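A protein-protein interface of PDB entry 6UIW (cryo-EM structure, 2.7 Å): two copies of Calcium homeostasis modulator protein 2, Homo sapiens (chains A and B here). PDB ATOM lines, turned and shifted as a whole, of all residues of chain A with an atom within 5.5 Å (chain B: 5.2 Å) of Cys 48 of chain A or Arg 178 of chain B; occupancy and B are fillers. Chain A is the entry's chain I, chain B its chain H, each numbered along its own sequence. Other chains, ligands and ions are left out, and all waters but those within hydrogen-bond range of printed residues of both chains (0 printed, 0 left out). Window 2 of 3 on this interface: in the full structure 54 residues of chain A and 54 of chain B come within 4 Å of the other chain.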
ATOM      1  N   CYS A  46      13.576  -9.959 -16.071  1.00  0.00           N
ATOM      2  CA  CYS A  46      12.978  -8.757 -15.530  1.00  0.00           C
ATOM      3  C   CYS A  46      11.501  -8.692 -15.856  1.00  0.00           C
ATOM      4  O   CYS A  46      11.126  -8.830 -17.027  1.00  0.00           O
ATOM      5  CB  CYS A  46      13.668  -7.516 -16.076  1.00  0.00           C
ATOM      6  SG  CYS A  46      12.984  -6.010 -15.377  1.00  0.00           S
ATOM      7  N   PRO A  47      10.636  -8.490 -14.862  1.00  0.00           N
ATOM      8  CA  PRO A  47       9.228  -8.204 -15.149  1.00  0.00           C
ATOM      9  C   PRO A  47       9.082  -6.764 -15.592  1.00  0.00           C
ATOM     10  O   PRO A  47       9.112  -5.840 -14.777  1.00  0.00           O
ATOM     11  CB  PRO A  47       8.538  -8.444 -13.809  1.00  0.00           C
ATOM     12  CG  PRO A  47       9.576  -8.313 -12.799  1.00  0.00           C
ATOM     13  CD  PRO A  47      10.916  -8.503 -13.423  1.00  0.00           C
ATOM     14  N   CYS A  48       8.895  -6.562 -16.882  1.00  0.00           N
ATOM     15  CA  CYS A  48       8.830  -5.204 -17.390  1.00  0.00           C
ATOM     16  C   CYS A  48       7.448  -4.632 -17.074  1.00  0.00           C
ATOM     17  O   CYS A  48       6.532  -4.601 -17.899  1.00  0.00           O
ATOM     18  CB  CYS A  48       9.173  -5.209 -18.866  1.00  0.00           C
ATOM     19  SG  CYS A  48      10.957  -5.188 -19.082  1.00  0.00           S
ATOM     20  N   SER A  49       7.310  -4.186 -15.830  1.00  0.00           N
ATOM     21  CA  SER A  49       6.070  -3.680 -15.271  1.00  0.00           C
ATOM     22  C   SER A  49       6.395  -2.843 -14.050  1.00  0.00           C
ATOM     23  O   SER A  49       7.311  -3.183 -13.291  1.00  0.00           O
ATOM     24  CB  SER A  49       5.122  -4.824 -14.878  1.00  0.00           C
ATOM     25  N   PRO A  50       5.673  -1.749 -13.825  1.00  0.00           N
ATOM     26  CA  PRO A  50       5.975  -0.892 -12.678  1.00  0.00           C
ATOM     27  C   PRO A  50       5.523  -1.526 -11.378  1.00  0.00           C
ATOM     28  O   PRO A  50       4.661  -2.407 -11.367  1.00  0.00           O
ATOM     29  CB  PRO A  50       5.184   0.381 -12.973  1.00  0.00           C
ATOM     30  CG  PRO A  50       4.030  -0.110 -13.742  1.00  0.00           C
ATOM     31  CD  PRO A  50       4.579  -1.189 -14.632  1.00  0.00           C
ATOM     32  N   ASN A  53       9.018  -4.706 -10.565  1.00  0.00           N
ATOM     33  CA  ASN A  53      10.340  -5.130 -10.988  1.00  0.00           C
ATOM     34  C   ASN A  53      11.390  -4.815  -9.941  1.00  0.00           C
ATOM     35  O   ASN A  53      12.431  -5.478  -9.881  1.00  0.00           O
ATOM     36  CB  ASN A  53      10.693  -4.492 -12.322  1.00  0.00           C
ATOM     37  CG  ASN A  53      10.313  -3.052 -12.390  1.00  0.00           C
ATOM     38  OD1 ASN A  53       9.928  -2.454 -11.392  1.00  0.00           O
ATOM     39  ND2 ASN A  53      10.414  -2.473 -13.574  1.00  0.00           N
ATOM     40  N   GLU A 155       4.810   3.070 -16.919  1.00  0.00           N
ATOM     41  CA  GLU A 155       4.742   1.746 -17.525  1.00  0.00           C
ATOM     42  C   GLU A 155       5.712   1.617 -18.691  1.00  0.00           C
ATOM     43  O   GLU A 155       6.424   0.611 -18.809  1.00  0.00           O
ATOM     44  CB  GLU A 155       3.313   1.450 -17.973  1.00  0.00           C
ATOM     45  N   ALA A 158       9.109   1.429 -17.238  1.00  0.00           N
ATOM     46  CA  ALA A 158       9.407   0.133 -16.647  1.00  0.00           C
ATOM     47  C   ALA A 158       9.550  -0.960 -17.685  1.00  0.00           C
ATOM     48  O   ALA A 158      10.107  -2.016 -17.382  1.00  0.00           O
ATOM     49  CB  ALA A 158       8.317  -0.245 -15.652  1.00  0.00           C
ATOM     50  N   ARG A 159       9.063  -0.739 -18.898  1.00  0.00           N
ATOM     51  CA  ARG A 159       9.195  -1.736 -19.946  1.00  0.00           C
ATOM     52  C   ARG A 159      10.519  -1.620 -20.696  1.00  0.00           C
ATOM     53  O   ARG A 159      10.799  -2.450 -21.566  1.00  0.00           O
ATOM     54  CB  ARG A 159       8.000  -1.637 -20.897  1.00  0.00           C
ATOM     55  CG  ARG A 159       7.603  -2.954 -21.528  1.00  0.00           C
ATOM     56  CD  ARG A 159       6.246  -2.874 -22.194  1.00  0.00           C
ATOM     57  NE  ARG A 159       5.189  -2.628 -21.223  1.00  0.00           N
ATOM     58  CZ  ARG A 159       4.326  -1.621 -21.296  1.00  0.00           C
ATOM     59  NH1 ARG A 159       3.395  -1.474 -20.364  1.00  0.00           N
ATOM     60  NH2 ARG A 159       4.385  -0.767 -22.307  1.00  0.00           N
ATOM     61  N   PHE A 160      11.343  -0.627 -20.357  1.00  0.00           N
ATOM     62  CA  PHE A 160      12.646  -0.460 -21.005  1.00  0.00           C
ATOM     63  C   PHE A 160      13.636  -1.619 -20.876  1.00  0.00           C
ATOM     64  O   PHE A 160      14.278  -1.931 -21.893  1.00  0.00           O
ATOM     65  CB  PHE A 160      13.322   0.829 -20.514  1.00  0.00           C
ATOM     66  CG  PHE A 160      12.788   2.079 -21.135  1.00  0.00           C
ATOM     67  CD1 PHE A 160      12.019   2.030 -22.280  1.00  0.00           C
ATOM     68  CD2 PHE A 160      13.077   3.312 -20.579  1.00  0.00           C
ATOM     69  CE1 PHE A 160      11.542   3.188 -22.849  1.00  0.00           C
ATOM     70  CE2 PHE A 160      12.608   4.471 -21.151  1.00  0.00           C
ATOM     71  CZ  PHE A 160      11.829   4.407 -22.281  1.00  0.00           C
ATOM     72  N   PRO A 161      13.855  -2.271 -19.712  1.00  0.00           N
ATOM     73  CA  PRO A 161      14.957  -3.254 -19.665  1.00  0.00           C
ATOM     74  C   PRO A 161      14.719  -4.536 -20.442  1.00  0.00           C
ATOM     75  O   PRO A 161      15.651  -5.331 -20.595  1.00  0.00           O
ATOM     76  CB  PRO A 161      15.099  -3.535 -18.165  1.00  0.00           C
ATOM     77  CG  PRO A 161      13.788  -3.241 -17.625  1.00  0.00           C
ATOM     78  CD  PRO A 161      13.367  -2.033 -18.340  1.00  0.00           C
ATOM     79  N   CYS A 162      13.508  -4.763 -20.952  1.00  0.00           N
ATOM     80  CA  CYS A 162      13.283  -5.936 -21.787  1.00  0.00           C
ATOM     81  C   CYS A 162      13.572  -5.642 -23.250  1.00  0.00           C
ATOM     82  O   CYS A 162      13.269  -6.474 -24.114  1.00  0.00           O
ATOM     83  CB  CYS A 162      11.845  -6.424 -21.638  1.00  0.00           C
ATOM     84  SG  CYS A 162      11.401  -6.945 -19.980  1.00  0.00           S
ATOM     85  N   GLU A 164      11.849  -3.516 -24.815  1.00  0.00           N
ATOM     86  CA  GLU A 164      10.503  -3.446 -25.354  1.00  0.00           C
ATOM     87  C   GLU A 164      10.019  -2.018 -25.519  1.00  0.00           C
ATOM     88  O   GLU A 164       8.810  -1.774 -25.466  1.00  0.00           O
ATOM     89  CB  GLU A 164       9.534  -4.223 -24.461  1.00  0.00           C
ATOM     90  N   ARG B 173       0.214 -11.261 -24.712  1.00  0.00           N
ATOM     91  CA  ARG B 173       0.722 -12.551 -24.264  1.00  0.00           C
ATOM     92  C   ARG B 173       2.097 -12.413 -23.633  1.00  0.00           C
ATOM     93  O   ARG B 173       2.387 -13.067 -22.628  1.00  0.00           O
ATOM     94  CB  ARG B 173       0.766 -13.538 -25.428  1.00  0.00           C
ATOM     95  CG  ARG B 173       1.280 -14.905 -25.043  1.00  0.00           C
ATOM     96  CD  ARG B 173       1.394 -15.812 -26.234  1.00  0.00           C
ATOM     97  NE  ARG B 173       2.714 -15.741 -26.844  1.00  0.00           N
ATOM     98  CZ  ARG B 173       2.917 -15.606 -28.148  1.00  0.00           C
ATOM     99  NH1 ARG B 173       1.884 -15.529 -28.975  1.00  0.00           N
ATOM    100  NH2 ARG B 173       4.151 -15.553 -28.626  1.00  0.00           N
ATOM    101  N   GLU B 174       2.945 -11.544 -24.188  1.00  0.00           N
ATOM    102  CA  GLU B 174       4.247 -11.300 -23.575  1.00  0.00           C
ATOM    103  C   GLU B 174       4.102 -10.611 -22.223  1.00  0.00           C
ATOM    104  O   GLU B 174       4.869 -10.896 -21.297  1.00  0.00           O
ATOM    105  CB  GLU B 174       5.124 -10.470 -24.506  1.00  0.00           C
ATOM    106  N   GLU B 175       3.095  -9.745 -22.077  1.00  0.00           N
ATOM    107  CA  GLU B 175       2.869  -9.084 -20.794  1.00  0.00           C
ATOM    108  C   GLU B 175       2.418 -10.069 -19.725  1.00  0.00           C
ATOM    109  O   GLU B 175       2.938 -10.054 -18.603  1.00  0.00           O
ATOM    110  CB  GLU B 175       1.841  -7.966 -20.947  1.00  0.00           C
ATOM    111  N   VAL B 176       1.466 -10.943 -20.058  1.00  0.00           N
ATOM    112  CA  VAL B 176       1.018 -11.952 -19.098  1.00  0.00           C
ATOM    113  C   VAL B 176       2.114 -12.965 -18.806  1.00  0.00           C
ATOM    114  O   VAL B 176       2.263 -13.409 -17.663  1.00  0.00           O
ATOM    115  CB  VAL B 176      -0.267 -12.636 -19.585  1.00  0.00           C
ATOM    116  CG1 VAL B 176      -0.877 -13.412 -18.485  1.00  0.00           C
ATOM    117  CG2 VAL B 176      -1.268 -11.601 -19.922  1.00  0.00           C
ATOM    118  N   SER B 177       2.915 -13.317 -19.812  1.00  0.00           N
ATOM    119  CA  SER B 177       4.010 -14.253 -19.587  1.00  0.00           C
ATOM    120  C   SER B 177       5.049 -13.669 -18.649  1.00  0.00           C
ATOM    121  O   SER B 177       5.497 -14.347 -17.722  1.00  0.00           O
ATOM    122  CB  SER B 177       4.660 -14.638 -20.909  1.00  0.00           C
ATOM    123  OG  SER B 177       5.995 -15.053 -20.686  1.00  0.00           O
ATOM    124  N   ARG B 178       5.386 -12.391 -18.819  1.00  0.00           N
ATOM    125  CA  ARG B 178       6.376 -11.779 -17.944  1.00  0.00           C
ATOM    126  C   ARG B 178       5.828 -11.572 -16.541  1.00  0.00           C
ATOM    127  O   ARG B 178       6.545 -11.793 -15.563  1.00  0.00           O
ATOM    128  CB  ARG B 178       6.860 -10.459 -18.536  1.00  0.00           C
ATOM    129  CG  ARG B 178       7.962 -10.638 -19.548  1.00  0.00           C
ATOM    130  CD  ARG B 178       8.610  -9.319 -19.886  1.00  0.00           C
ATOM    131  NE  ARG B 178       7.978  -8.666 -21.025  1.00  0.00           N
ATOM    132  CZ  ARG B 178       7.047  -7.725 -20.927  1.00  0.00           C
ATOM    133  NH1 ARG B 178       6.532  -7.188 -22.021  1.00  0.00           N
ATOM    134  NH2 ARG B 178       6.631  -7.315 -19.739  1.00  0.00           N
ATOM    135  N   ARG B 179       4.546 -11.213 -16.419  1.00  0.00           N
ATOM    136  CA  ARG B 179       3.970 -10.979 -15.097  1.00  0.00           C
ATOM    137  C   ARG B 179       3.848 -12.275 -14.303  1.00  0.00           C
ATOM    138  O   ARG B 179       4.197 -12.334 -13.117  1.00  0.00           O
ATOM    139  CB  ARG B 179       2.606 -10.312 -15.234  1.00  0.00           C
ATOM    140  CG  ARG B 179       1.809 -10.324 -13.957  1.00  0.00           C
ATOM    141  CD  ARG B 179       0.375  -9.949 -14.191  1.00  0.00           C
ATOM    142  NE  ARG B 179       0.273  -8.702 -14.933  1.00  0.00           N
ATOM    143  CZ  ARG B 179      -0.827  -7.964 -14.995  1.00  0.00           C
ATOM    144  NH1 ARG B 179      -1.923  -8.349 -14.362  1.00  0.00           N
ATOM    145  NH2 ARG B 179      -0.827  -6.839 -15.695  1.00  0.00           N
ATOM    146  N   LEU B 180       3.388 -13.341 -14.947  1.00  0.00           N
ATOM    147  CA  LEU B 180       3.209 -14.583 -14.213  1.00  0.00           C
ATOM    148  C   LEU B 180       4.533 -15.302 -14.007  1.00  0.00           C
ATOM    149  O   LEU B 180       4.700 -16.018 -13.017  1.00  0.00           O
ATOM    150  CB  LEU B 180       2.212 -15.471 -14.931  1.00  0.00           C
ATOM    151  CG  LEU B 180       0.776 -15.001 -15.033  1.00  0.00           C
ATOM    152  CD1 LEU B 180       0.009 -16.142 -15.609  1.00  0.00           C
ATOM    153  CD2 LEU B 180       0.203 -14.582 -13.687  1.00  0.00           C
ATOM    154  N   ARG B 181       5.503 -15.107 -14.905  1.00  0.00           N
ATOM    155  CA  ARG B 181       6.835 -15.629 -14.645  1.00  0.00           C
ATOM    156  C   ARG B 181       7.501 -14.869 -13.511  1.00  0.00           C
ATOM    157  O   ARG B 181       8.276 -15.446 -12.739  1.00  0.00           O
ATOM    158  CB  ARG B 181       7.680 -15.558 -15.909  1.00  0.00           C
ATOM    159  CG  ARG B 181       8.981 -16.307 -15.815  1.00  0.00           C
ATOM    160  CD  ARG B 181       9.728 -16.271 -17.127  1.00  0.00           C
ATOM    161  NE  ARG B 181      10.374 -14.982 -17.348  1.00  0.00           N
ATOM    162  CZ  ARG B 181      10.034 -14.128 -18.308  1.00  0.00           C
ATOM    163  NH1 ARG B 181       9.054 -14.425 -19.146  1.00  0.00           N
ATOM    164  NH2 ARG B 181      10.680 -12.977 -18.435  1.00  0.00           N
ATOM    165  N   TYR B 182       7.187 -13.577 -13.378  1.00  0.00           N
ATOM    166  CA  TYR B 182       7.613 -12.821 -12.208  1.00  0.00           C
ATOM    167  C   TYR B 182       7.036 -13.406 -10.940  1.00  0.00           C
ATOM    168  O   TYR B 182       7.755 -13.573  -9.956  1.00  0.00           O
ATOM    169  CB  TYR B 182       7.185 -11.365 -12.326  1.00  0.00           C
ATOM    170  CG  TYR B 182       6.877 -10.684 -11.006  1.00  0.00           C
ATOM    171  CD1 TYR B 182       7.891 -10.262 -10.163  1.00  0.00           C
ATOM    172  CD2 TYR B 182       5.566 -10.447 -10.615  1.00  0.00           C
ATOM    173  CE1 TYR B 182       7.609  -9.653  -8.962  1.00  0.00           C
ATOM    174  CE2 TYR B 182       5.278  -9.844  -9.414  1.00  0.00           C
ATOM    175  CZ  TYR B 182       6.303  -9.440  -8.599  1.00  0.00           C
ATOM    176  OH  TYR B 182       6.014  -8.828  -7.407  1.00  0.00           O
ATOM    177  N   GLU B 183       5.730 -13.674 -10.929  1.00  0.00           N
ATOM    178  CA  GLU B 183       5.102 -14.177  -9.713  1.00  0.00           C
ATOM    179  C   GLU B 183       5.592 -15.581  -9.390  1.00  0.00           C
ATOM    180  O   GLU B 183       5.743 -15.937  -8.218  1.00  0.00           O
ATOM    181  CB  GLU B 183       3.583 -14.140  -9.853  1.00  0.00           C
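The side-chain sulfur (SG) of Cys 48 of chain A forms a disulfide with the side-chain sulfur (SG) of Cys 162 of chain A (2.0 Å).
Among the printed residues, pairs that only touch across the chains: Cys 46 of chain A with Arg 178 of chain B (3.8 Å), Pro 47 of chain A with Tyr 182 of chain B (3.5 Å) and Cys 162 of chain A with Arg 178 of chain B (3.7 Å).
Of the 11 printed residues of chain B, 2 touch a printed residue of chain A. Hydrophobic or aromatic side chains of chain B within 4 Å of the printed part of chain A: Tyr 182. Of the 13 printed residues of chain A, 4 touch a printed residue of chain B.
Of the printed residues of chain B, Pro 47 of chain A touches Tyr 182. Printed residues of chain B within 4 Å of Cys 48 of chain A: Arg 178. Arg 178 of chain B touches just these residues of chain A: Cys 46, Cys 48 and Cys 162. Arg 181 of chain B touches none of the printed residues of chain A. Of the printed residues of chain A, Tyr 182 of chain B touches Pro 47. The nearest printed residue of chain B that does not touch Cys 46 of chain A is Arg 181 of chain B (4.4 Å).
No position is printed for both chains. Of the 4 pairs that touch across the chains among the printed residues, none has its exchanged pair printed and touching as well.
O of Cys 48 of chain A is in hydrogen-bond range of NH2 of Arg 178 of chain B.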
